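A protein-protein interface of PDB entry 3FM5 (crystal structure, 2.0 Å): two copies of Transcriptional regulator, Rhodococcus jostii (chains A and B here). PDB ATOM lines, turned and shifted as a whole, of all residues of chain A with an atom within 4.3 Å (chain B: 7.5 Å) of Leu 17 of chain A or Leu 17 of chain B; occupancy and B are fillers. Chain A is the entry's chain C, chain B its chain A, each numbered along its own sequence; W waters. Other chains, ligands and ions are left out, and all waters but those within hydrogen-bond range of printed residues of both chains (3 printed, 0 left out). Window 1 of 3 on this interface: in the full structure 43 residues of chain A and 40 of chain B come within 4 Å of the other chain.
Ile 13 of chain A touches Phe 123 of chain B, and with the chains exchanged Phe 123 of chain A touches Ile 13 of chain B. Leu 17 of chain A touches its own counterpart, Leu 17 of chain B. Val 20 of chain A touches Leu 17 of chain B, but with the chains exchanged Leu 17 of chain A does not touch Val 20 of chain B (4.05 Å). Val 20 of chain A touches Leu 138 of chain B, and with the chains exchanged Leu 138 of chain A touches Val 20 of chain B. Positions printed for both chains: 13, 14, 15, 16, 17, 18, 19, 20, 21, 123 and 138. Of the 23 pairs that touch across the chains among the printed residues, 13 have their exchanged pair printed and touching as well.
O of Gly 14 of chain A sits at hydrogen-bond distance from OG of Ser 18 of chain A, at 3.2 Å.
Of the printed residues of chain B, Leu 17 of chain A touches Leu 17, Phe 123 and Leu 138. Of the printed residues of chain A, Leu 17 of chain B touches Leu 17 (3.9 Å), Val 20 (3.9 Å), Phe 123 (3.98 Å) and Leu 138 (3.6 Å). Printed residues of chain A within 4 Å of Ala 142 of chain B: Arg 19 (3.97 Å) and Val 20 (3.8 Å). Of the printed residues of chain B, Ile 13 of chain A touches His 119, Phe 123, Met 134 and Leu 138. Of the printed residues of chain A, Ile 141 of chain B touches Val 20 (3.9 Å) and Phe 123 (3.5 Å). Ser 18 of chain B touches none of the printed residues of chain A. Leu 25 of chain B touches none of the printed residues of chain A. The nearest printed residue of chain B that does not touch Leu 17 of chain A is Gly 21 of chain B (4.04 Å). The nearest printed residue of chain B that does not touch Val 20 of chain A is Thr 137 of chain B (5.8 Å).
Of the 21 printed residues of chain B, 11 touch a printed residue of chain A. Printed residues of chain B that touch a printed residue of chain A: Ile 13, Leu 16, Leu 17, Val 20, Val 24, His 119, Phe 123, Met 134, Leu 138, Ile 141 and Ala 142. Hydrophobic or aromatic side chains of chain A within 4 Å of the printed part of chain B: Ile 13, Leu 16, Leu 17, Val 20, Phe 123 and Leu 138. Among the printed residues, 23 pairs touch across the chains. Among the printed residues, no Asp or Glu carboxylate lies within 4 Å of a Lys or Arg side-chain nitrogen of the other chain.
Water W2 bridges O of Leu 17 of chain A (2.8 Å) and O of Leu 17 of chain B (3.0 Å). Water W1 lies within hydrogen-bond range of O of Gly 14 of chain A, O of Gly 21 of chain B and OG of Ser 18 of chain A. Water W3 lies within hydrogen-bond range of the side-chain hydroxyl (OG) of Ser 18 of chain A (2.9 Å), the backbone carbonyl oxygen (O) of Gly 21 of chain B (3.2 Å) and the backbone NH (N) of Gly 22 of chain B (3.3 Å).
Among the printed residues, pairs that only touch across the chains: Ile 13 of chain A with His 119 of chain B (3.7 Å), Ile 13 of chain A with Phe 123 of chain B (3.8 Å), Ile 13 of chain A with Met 134 of chain B (3.6 Å), Ile 13 of chain A with Leu 138 of chain B (3.96 Å), Gly 14 of chain A with Val 24 of chain B (3.98 Å), Gly 14 of chain A with His 119 of chain B (3.9 Å), Leu 16 of chain A with Leu 138 of chain B (3.8 Å), Leu 17 of chain A with Leu 17 of chain B (3.9 Å), Leu 17 of chain A with Phe 123 of chain B (3.999 Å), Leu 17 of chain A with Leu 138 of chain B (3.8 Å), Arg 19 of chain A with Ala 142 of chain B (3.97 Å), Val 20 of chain A with Leu 17 of chain B (3.9 Å), Val 20 of chain A with Leu 138 of chain B (3.5 Å), Val 20 of chain A with Ile 141 of chain B (3.9 Å), Val 20 of chain A with Ala 142 of chain B (3.8 Å), Phe 123 of chain A with Ile 13 of chain B (3.6 Å), Phe 123 of chain A with Leu 17 of chain B (3.98 Å), Phe 123 of chain A with Ile 141 of chain B (3.5 Å), Leu 138 of chain A with Ile 13 of chain B (3.9 Å), Leu 138 of chain A with Leu 16 of chain B (3.7 Å), Leu 138 of chain A with Leu 17 of chain B (3.6 Å), Leu 138 of chain A with Val 20 of chain B (3.5 Å) and Leu 138 of chain A with Met 134 of chain B (3.8 Å).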
ATOM      1  N   ILE A  13       0.348   5.076  -0.801  1.00  0.00           N
ATOM      2  CA  ILE A  13       0.513   3.793  -1.477  1.00  0.00           C
ATOM      3  C   ILE A  13       1.022   3.957  -2.914  1.00  0.00           C
ATOM      4  O   ILE A  13       1.802   3.140  -3.400  1.00  0.00           O
ATOM      5  CB  ILE A  13      -0.803   2.973  -1.474  1.00  0.00           C
ATOM      6  CG1 ILE A  13      -0.534   1.521  -1.873  1.00  0.00           C
ATOM      7  CG2 ILE A  13      -1.843   3.605  -2.393  1.00  0.00           C
ATOM      8  CD1 ILE A  13       0.163   0.719  -0.797  1.00  0.00           C
ATOM      9  N   GLY A  14       0.577   5.014  -3.586  1.00  0.00           N
ATOM     10  CA  GLY A  14       1.035   5.301  -4.936  1.00  0.00           C
ATOM     11  C   GLY A  14       2.502   5.680  -4.937  1.00  0.00           C
ATOM     12  O   GLY A  14       3.282   5.199  -5.766  1.00  0.00           O
ATOM     13  N   PHE A  15       2.881   6.544  -3.998  1.00  0.00           N
ATOM     14  CA  PHE A  15       4.281   6.926  -3.819  1.00  0.00           C
ATOM     15  C   PHE A  15       5.153   5.695  -3.604  1.00  0.00           C
ATOM     16  O   PHE A  15       6.210   5.551  -4.220  1.00  0.00           O
ATOM     17  CB  PHE A  15       4.426   7.878  -2.631  1.00  0.00           C
ATOM     18  CG  PHE A  15       5.853   8.158  -2.246  1.00  0.00           C
ATOM     19  CD1 PHE A  15       6.613   9.071  -2.957  1.00  0.00           C
ATOM     20  CD2 PHE A  15       6.434   7.509  -1.173  1.00  0.00           C
ATOM     21  CE1 PHE A  15       7.923   9.332  -2.600  1.00  0.00           C
ATOM     22  CE2 PHE A  15       7.746   7.766  -0.813  1.00  0.00           C
ATOM     23  CZ  PHE A  15       8.489   8.677  -1.528  1.00  0.00           C
ATOM     24  N   LEU A  16       4.697   4.801  -2.735  1.00  0.00           N
ATOM     25  CA  LEU A  16       5.459   3.610  -2.388  1.00  0.00           C
ATOM     26  C   LEU A  16       5.600   2.669  -3.582  1.00  0.00           C
ATOM     27  O   LEU A  16       6.684   2.144  -3.846  1.00  0.00           O
ATOM     28  CB  LEU A  16       4.799   2.887  -1.212  1.00  0.00           C
ATOM     29  CG  LEU A  16       4.817   3.615   0.133  1.00  0.00           C
ATOM     30  CD1 LEU A  16       3.894   2.935   1.138  1.00  0.00           C
ATOM     31  CD2 LEU A  16       6.240   3.728   0.674  1.00  0.00           C
ATOM     32  N   LEU A  17       4.507   2.462  -4.312  1.00  0.00           N
ATOM     33  CA  LEU A  17       4.553   1.614  -5.498  1.00  0.00           C
ATOM     34  C   LEU A  17       5.552   2.180  -6.510  1.00  0.00           C
ATOM     35  O   LEU A  17       6.361   1.448  -7.077  1.00  0.00           O
ATOM     36  CB  LEU A  17       3.165   1.472  -6.135  1.00  0.00           C
ATOM     37  CG  LEU A  17       2.147   0.619  -5.368  1.00  0.00           C
ATOM     38  CD1 LEU A  17       0.728   0.901  -5.858  1.00  0.00           C
ATOM     39  CD2 LEU A  17       2.466  -0.869  -5.481  1.00  0.00           C
ATOM     40  N   SER A  18       5.505   3.487  -6.725  1.00  0.00           N
ATOM     41  CA  SER A  18       6.382   4.103  -7.717  1.00  0.00           C
ATOM     42  C   SER A  18       7.845   4.078  -7.265  1.00  0.00           C
ATOM     43  O   SER A  18       8.743   3.799  -8.059  1.00  0.00           O
ATOM     44  CB  SER A  18       5.923   5.527  -8.044  1.00  0.00           C
ATOM     45  OG  SER A  18       4.635   5.506  -8.636  1.00  0.00           O
ATOM     46  N   ARG A  19       8.080   4.339  -5.985  1.00  0.00           N
ATOM     47  CA  ARG A  19       9.437   4.295  -5.439  1.00  0.00           C
ATOM     48  C   ARG A  19      10.029   2.881  -5.503  1.00  0.00           C
ATOM     49  O   ARG A  19      11.127   2.683  -6.017  1.00  0.00           O
ATOM     50  CB  ARG A  19       9.458   4.824  -4.001  1.00  0.00           C
ATOM     51  CG  ARG A  19      10.832   4.827  -3.351  1.00  0.00           C
ATOM     52  CD  ARG A  19      11.771   5.817  -4.023  1.00  0.00           C
ATOM     53  NE  ARG A  19      13.054   5.888  -3.331  1.00  0.00           N
ATOM     54  CZ  ARG A  19      13.276   6.620  -2.243  1.00  0.00           C
ATOM     55  NH1 ARG A  19      12.300   7.350  -1.722  1.00  0.00           N
ATOM     56  NH2 ARG A  19      14.475   6.623  -1.674  1.00  0.00           N
ATOM     57  N   VAL A  20       9.295   1.897  -4.995  1.00  0.00           N
ATOM     58  CA  VAL A  20       9.774   0.515  -5.006  1.00  0.00           C
ATOM     59  C   VAL A  20       9.866  -0.054  -6.426  1.00  0.00           C
ATOM     60  O   VAL A  20      10.834  -0.730  -6.770  1.00  0.00           O
ATOM     61  CB  VAL A  20       8.909  -0.406  -4.118  1.00  0.00           C
ATOM     62  CG1 VAL A  20       9.385  -1.853  -4.229  1.00  0.00           C
ATOM     63  CG2 VAL A  20       8.966   0.055  -2.669  1.00  0.00           C
ATOM     64  N   GLY A  21       8.868   0.235  -7.254  1.00  0.00           N
ATOM     65  CA  GLY A  21       8.915  -0.159  -8.651  1.00  0.00           C
ATOM     66  C   GLY A  21      10.150   0.367  -9.368  1.00  0.00           C
ATOM     67  O   GLY A  21      10.803  -0.359 -10.126  1.00  0.00           O
ATOM     68  N   PHE A 123      13.746  -8.633  -2.027  1.00  0.00           N
ATOM     69  CA  PHE A 123      12.685  -9.451  -1.433  1.00  0.00           C
ATOM     70  C   PHE A 123      13.130 -10.555  -0.478  1.00  0.00           C
ATOM     71  O   PHE A 123      12.347 -11.003   0.359  1.00  0.00           O
ATOM     72  CB  PHE A 123      11.767 -10.013  -2.519  1.00  0.00           C
ATOM     73  CG  PHE A 123      10.999  -8.956  -3.239  1.00  0.00           C
ATOM     74  CD1 PHE A 123      11.377  -8.547  -4.506  1.00  0.00           C
ATOM     75  CD2 PHE A 123       9.924  -8.333  -2.629  1.00  0.00           C
ATOM     76  CE1 PHE A 123      10.676  -7.550  -5.166  1.00  0.00           C
ATOM     77  CE2 PHE A 123       9.218  -7.336  -3.282  1.00  0.00           C
ATOM     78  CZ  PHE A 123       9.597  -6.943  -4.553  1.00  0.00           C
ATOM     79  N   LEU A 138      -1.571  -7.167  -6.475  1.00  0.00           N
ATOM     80  CA  LEU A 138      -1.161  -6.450  -7.679  1.00  0.00           C
ATOM     81  C   LEU A 138      -1.786  -7.084  -8.919  1.00  0.00           C
ATOM     82  O   LEU A 138      -2.162  -6.392  -9.871  1.00  0.00           O
ATOM     83  CB  LEU A 138       0.364  -6.430  -7.819  1.00  0.00           C
ATOM     84  CG  LEU A 138       1.161  -5.668  -6.759  1.00  0.00           C
ATOM     85  CD1 LEU A 138       2.657  -5.788  -7.052  1.00  0.00           C
ATOM     86  CD2 LEU A 138       0.743  -4.212  -6.691  1.00  0.00           C
ATOM     87  N   ASP B  12       5.705 -12.149 -12.421  1.00  0.00           N
ATOM     88  CA  ASP B  12       6.911 -11.342 -12.258  1.00  0.00           C
ATOM     89  C   ASP B  12       6.606 -10.124 -11.383  1.00  0.00           C
ATOM     90  O   ASP B  12       5.949  -9.180 -11.825  1.00  0.00           O
ATOM     91  CB  ASP B  12       7.421 -10.920 -13.645  1.00  0.00           C
ATOM     92  CG  ASP B  12       8.631 -10.010 -13.591  1.00  0.00           C
ATOM     93  OD1 ASP B  12       9.452 -10.082 -14.531  1.00  0.00           O
ATOM     94  OD2 ASP B  12       8.760  -9.220 -12.629  1.00  0.00           O
ATOM     95  N   ILE B  13       7.106 -10.140 -10.150  1.00  0.00           N
ATOM     96  CA  ILE B  13       6.768  -9.103  -9.171  1.00  0.00           C
ATOM     97  C   ILE B  13       7.231  -7.702  -9.569  1.00  0.00           C
ATOM     98  O   ILE B  13       6.580  -6.720  -9.233  1.00  0.00           O
ATOM     99  CB  ILE B  13       7.301  -9.438  -7.756  1.00  0.00           C
ATOM    100  CG1 ILE B  13       6.702  -8.489  -6.718  1.00  0.00           C
ATOM    101  CG2 ILE B  13       8.821  -9.375  -7.714  1.00  0.00           C
ATOM    102  CD1 ILE B  13       5.215  -8.683  -6.497  1.00  0.00           C
ATOM    103  N   GLY B  14       8.362  -7.609 -10.267  1.00  0.00           N
ATOM    104  CA  GLY B  14       8.837  -6.330 -10.763  1.00  0.00           C
ATOM    105  C   GLY B  14       7.886  -5.769 -11.812  1.00  0.00           C
ATOM    106  O   GLY B  14       7.523  -4.589 -11.787  1.00  0.00           O
ATOM    107  N   PHE B  15       7.483  -6.619 -12.747  1.00  0.00           N
ATOM    108  CA  PHE B  15       6.518  -6.216 -13.760  1.00  0.00           C
ATOM    109  C   PHE B  15       5.224  -5.709 -13.129  1.00  0.00           C
ATOM    110  O   PHE B  15       4.689  -4.670 -13.525  1.00  0.00           O
ATOM    111  CB  PHE B  15       6.203  -7.373 -14.707  1.00  0.00           C
ATOM    112  CG  PHE B  15       5.076  -7.076 -15.654  1.00  0.00           C
ATOM    113  CD1 PHE B  15       5.276  -6.252 -16.750  1.00  0.00           C
ATOM    114  CD2 PHE B  15       3.812  -7.595 -15.433  1.00  0.00           C
ATOM    115  CE1 PHE B  15       4.239  -5.963 -17.617  1.00  0.00           C
ATOM    116  CE2 PHE B  15       2.766  -7.309 -16.300  1.00  0.00           C
ATOM    117  CZ  PHE B  15       2.983  -6.491 -17.392  1.00  0.00           C
ATOM    118  N   LEU B  16       4.725  -6.452 -12.147  1.00  0.00           N
ATOM    119  CA  LEU B  16       3.470  -6.108 -11.477  1.00  0.00           C
ATOM    120  C   LEU B  16       3.537  -4.766 -10.771  1.00  0.00           C
ATOM    121  O   LEU B  16       2.605  -3.963 -10.870  1.00  0.00           O
ATOM    122  CB  LEU B  16       3.079  -7.192 -10.470  1.00  0.00           C
ATOM    123  CG  LEU B  16       2.633  -8.524 -11.061  1.00  0.00           C
ATOM    124  CD1 LEU B  16       2.506  -9.565  -9.951  1.00  0.00           C
ATOM    125  CD2 LEU B  16       1.313  -8.374 -11.807  1.00  0.00           C
ATOM    126  N   LEU B  17       4.632  -4.539 -10.042  1.00  0.00           N
ATOM    127  CA  LEU B  17       4.857  -3.274  -9.351  1.00  0.00           C
ATOM    128  C   LEU B  17       4.843  -2.089 -10.315  1.00  0.00           C
ATOM    129  O   LEU B  17       4.216  -1.064 -10.050  1.00  0.00           O
ATOM    130  CB  LEU B  17       6.195  -3.299  -8.601  1.00  0.00           C
ATOM    131  CG  LEU B  17       6.203  -4.111  -7.305  1.00  0.00           C
ATOM    132  CD1 LEU B  17       7.625  -4.297  -6.783  1.00  0.00           C
ATOM    133  CD2 LEU B  17       5.311  -3.456  -6.257  1.00  0.00           C
ATOM    134  N   SER B  18       5.551  -2.221 -11.429  1.00  0.00           N
ATOM    135  CA  SER B  18       5.649  -1.105 -12.362  1.00  0.00           C
ATOM    136  C   SER B  18       4.331  -0.909 -13.090  1.00  0.00           C
ATOM    137  O   SER B  18       3.908   0.222 -13.341  1.00  0.00           O
ATOM    138  CB  SER B  18       6.785  -1.325 -13.362  1.00  0.00           C
ATOM    139  OG  SER B  18       6.503  -2.426 -14.202  1.00  0.00           O
ATOM    140  N   ARG B  19       3.672  -2.013 -13.425  1.00  0.00           N
ATOM    141  CA  ARG B  19       2.391  -1.930 -14.112  1.00  0.00           C
ATOM    142  C   ARG B  19       1.368  -1.216 -13.220  1.00  0.00           C
ATOM    143  O   ARG B  19       0.759  -0.229 -13.628  1.00  0.00           O
ATOM    144  CB  ARG B  19       1.899  -3.325 -14.510  1.00  0.00           C
ATOM    145  CG  ARG B  19       0.654  -3.326 -15.376  1.00  0.00           C
ATOM    146  CD  ARG B  19       0.943  -2.805 -16.782  1.00  0.00           C
ATOM    147  NE  ARG B  19      -0.221  -2.964 -17.651  1.00  0.00           N
ATOM    148  CZ  ARG B  19      -1.005  -1.970 -18.052  1.00  0.00           C
ATOM    149  NH1 ARG B  19      -2.041  -2.224 -18.838  1.00  0.00           N
ATOM    150  NH2 ARG B  19      -0.745  -0.722 -17.688  1.00  0.00           N
ATOM    151  N   VAL B  20       1.192  -1.706 -11.997  1.00  0.00           N
ATOM    152  CA  VAL B  20       0.224  -1.106 -11.075  1.00  0.00           C
ATOM    153  C   VAL B  20       0.624   0.305 -10.655  1.00  0.00           C
ATOM    154  O   VAL B  20      -0.219   1.202 -10.570  1.00  0.00           O
ATOM    155  CB  VAL B  20       0.005  -1.978  -9.829  1.00  0.00           C
ATOM    156  CG1 VAL B  20      -0.931  -1.276  -8.843  1.00  0.00           C
ATOM    157  CG2 VAL B  20      -0.556  -3.334 -10.242  1.00  0.00           C
ATOM    158  N   GLY B  21       1.914   0.502 -10.408  1.00  0.00           N
ATOM    159  CA  GLY B  21       2.422   1.824 -10.094  1.00  0.00           C
ATOM    160  C   GLY B  21       2.072   2.832 -11.177  1.00  0.00           C
ATOM    161  O   GLY B  21       1.639   3.944 -10.882  1.00  0.00           O
ATOM    162  N   GLY B  22       2.259   2.436 -12.434  1.00  0.00           N
ATOM    163  CA  GLY B  22       1.990   3.314 -13.562  1.00  0.00           C
ATOM    164  C   GLY B  22       0.511   3.646 -13.694  1.00  0.00           C
ATOM    165  O   GLY B  22       0.134   4.776 -14.010  1.00  0.00           O
ATOM    166  N   MET B  23      -0.333   2.650 -13.462  1.00  0.00           N
ATOM    167  CA  MET B  23      -1.779   2.852 -13.502  1.00  0.00           C
ATOM    168  C   MET B  23      -2.228   3.834 -12.422  1.00  0.00           C
ATOM    169  O   MET B  23      -2.976   4.770 -12.692  1.00  0.00           O
ATOM    170  CB  MET B  23      -2.502   1.515 -13.342  1.00  0.00           C
ATOM    171  CG  MET B  23      -2.271   0.560 -14.499  1.00  0.00           C
ATOM    172  SD  MET B  23      -2.852  -1.247 -14.072  1.00  0.00           S
ATOM    173  CE  MET B  23      -4.773  -0.931 -14.000  1.00  0.00           C
ATOM    174  N   VAL B  24      -1.758   3.629 -11.197  1.00  0.00           N
ATOM    175  CA  VAL B  24      -2.138   4.506 -10.095  1.00  0.00           C
ATOM    176  C   VAL B  24      -1.649   5.930 -10.329  1.00  0.00           C
ATOM    177  O   VAL B  24      -2.399   6.887 -10.145  1.00  0.00           O
ATOM    178  CB  VAL B  24      -1.624   3.980  -8.740  1.00  0.00           C
ATOM    179  CG1 VAL B  24      -1.880   4.997  -7.635  1.00  0.00           C
ATOM    180  CG2 VAL B  24      -2.289   2.650  -8.411  1.00  0.00           C
ATOM    181  N   LEU B  25      -0.393   6.066 -10.744  1.00  0.00           N
ATOM    182  CA  LEU B  25       0.177   7.382 -11.005  1.00  0.00           C
ATOM    183  C   LEU B  25      -0.657   8.128 -12.054  1.00  0.00           C
ATOM    184  O   LEU B  25      -0.928   9.325 -11.923  1.00  0.00           O
ATOM    185  CB  LEU B  25       1.630   7.240 -11.465  1.00  0.00           C
ATOM    186  CG  LEU B  25       2.349   8.477 -12.000  1.00  0.00           C
ATOM    187  CD1 LEU B  25       2.607   9.471 -10.883  1.00  0.00           C
ATOM    188  CD2 LEU B  25       3.657   8.066 -12.648  1.00  0.00           C
ATOM    189  N   HIS B 119      -6.950   6.499  -5.489  1.00  0.00           N
ATOM    190  CA  HIS B 119      -6.465   5.228  -4.951  1.00  0.00           C
ATOM    191  C   HIS B 119      -7.624   4.252  -4.768  1.00  0.00           C
ATOM    192  O   HIS B 119      -7.497   3.059  -5.041  1.00  0.00           O
ATOM    193  CB  HIS B 119      -5.765   5.421  -3.599  1.00  0.00           C
ATOM    194  CG  HIS B 119      -4.469   6.168  -3.674  1.00  0.00           C
ATOM    195  ND1 HIS B 119      -3.785   6.368  -4.856  1.00  0.00           N
ATOM    196  CD2 HIS B 119      -3.713   6.738  -2.706  1.00  0.00           C
ATOM    197  CE1 HIS B 119      -2.680   7.051  -4.616  1.00  0.00           C
ATOM    198  NE2 HIS B 119      -2.610   7.283  -3.317  1.00  0.00           N
ATOM    199  N   PHE B 123      -8.129   0.233  -5.252  1.00  0.00           N
ATOM    200  CA  PHE B 123      -7.984  -0.613  -4.069  1.00  0.00           C
ATOM    201  C   PHE B 123      -9.290  -0.982  -3.370  1.00  0.00           C
ATOM    202  O   PHE B 123      -9.337  -1.958  -2.628  1.00  0.00           O
ATOM    203  CB  PHE B 123      -6.987   0.011  -3.092  1.00  0.00           C
ATOM    204  CG  PHE B 123      -5.588   0.056  -3.626  1.00  0.00           C
ATOM    205  CD1 PHE B 123      -5.079   1.219  -4.178  1.00  0.00           C
ATOM    206  CD2 PHE B 123      -4.793  -1.075  -3.602  1.00  0.00           C
ATOM    207  CE1 PHE B 123      -3.792   1.257  -4.682  1.00  0.00           C
ATOM    208  CE2 PHE B 123      -3.501  -1.044  -4.103  1.00  0.00           C
ATOM    209  CZ  PHE B 123      -3.003   0.124  -4.646  1.00  0.00           C
ATOM    210  N   MET B 134       0.514  -4.539   2.391  1.00  0.00           N
ATOM    211  CA  MET B 134       1.349  -4.227   1.245  1.00  0.00           C
ATOM    212  C   MET B 134       2.089  -2.913   1.456  1.00  0.00           C
ATOM    213  O   MET B 134       3.261  -2.785   1.094  1.00  0.00           O
ATOM    214  CB  MET B 134       0.539  -4.157  -0.047  1.00  0.00           C
ATOM    215  CG  MET B 134       1.435  -3.894  -1.251  1.00  0.00           C
ATOM    216  SD  MET B 134       0.474  -3.978  -2.926  1.00  0.00           S
ATOM    217  CE  MET B 134      -0.463  -2.277  -2.772  1.00  0.00           C
ATOM    218  N   THR B 137       5.042  -3.643   3.635  1.00  0.00           N
ATOM    219  CA  THR B 137       6.160  -4.316   2.980  1.00  0.00           C
ATOM    220  C   THR B 137       6.866  -3.396   1.983  1.00  0.00           C
ATOM    221  O   THR B 137       8.091  -3.414   1.880  1.00  0.00           O
ATOM    222  CB  THR B 137       5.761  -5.661   2.320  1.00  0.00           C
ATOM    223  OG1 THR B 137       5.585  -5.488   0.916  1.00  0.00           O
ATOM    224  CG2 THR B 137       4.488  -6.215   2.942  1.00  0.00           C
ATOM    225  N   LEU B 138       6.098  -2.580   1.268  1.00  0.00           N
ATOM    226  CA  LEU B 138       6.693  -1.580   0.388  1.00  0.00           C
ATOM    227  C   LEU B 138       7.582  -0.626   1.188  1.00  0.00           C
ATOM    228  O   LEU B 138       8.683  -0.266   0.756  1.00  0.00           O
ATOM    229  CB  LEU B 138       5.609  -0.793  -0.348  1.00  0.00           C
ATOM    230  CG  LEU B 138       4.758  -1.577  -1.347  1.00  0.00           C
ATOM    231  CD1 LEU B 138       3.691  -0.666  -1.941  1.00  0.00           C
ATOM    232  CD2 LEU B 138       5.623  -2.183  -2.430  1.00  0.00           C
ATOM    233  N   ILE B 141      10.983  -2.002   2.098  1.00  0.00           N
ATOM    234  CA  ILE B 141      11.873  -2.016   0.941  1.00  0.00           C
ATOM    235  C   ILE B 141      12.361  -0.617   0.571  1.00  0.00           C
ATOM    236  O   ILE B 141      13.550  -0.405   0.351  1.00  0.00           O
ATOM    237  CB  ILE B 141      11.183  -2.621  -0.290  1.00  0.00           C
ATOM    238  CG1 ILE B 141      10.793  -4.075  -0.028  1.00  0.00           C
ATOM    239  CG2 ILE B 141      12.088  -2.516  -1.508  1.00  0.00           C
ATOM    240  CD1 ILE B 141       9.847  -4.638  -1.076  1.00  0.00           C
ATOM    241  N   ALA B 142      11.436   0.334   0.501  1.00  0.00           N
ATOM    242  CA  ALA B 142      11.771   1.700   0.107  1.00  0.00           C
ATOM    243  C   ALA B 142      12.627   2.395   1.152  1.00  0.00           C
ATOM    244  O   ALA B 142      13.569   3.106   0.814  1.00  0.00           O
ATOM    245  CB  ALA B 142      10.505   2.506  -0.151  1.00  0.00           C
HETATM  246  O   HOH W   1       1.850   4.881  -8.162  1.00  0.00           O
HETATM  247  O   HOH W   2       6.000   1.333  -9.841  1.00  0.00           O
HETATM  248  O   HOH W   3       4.773   4.139 -11.152  1.00  0.00           O
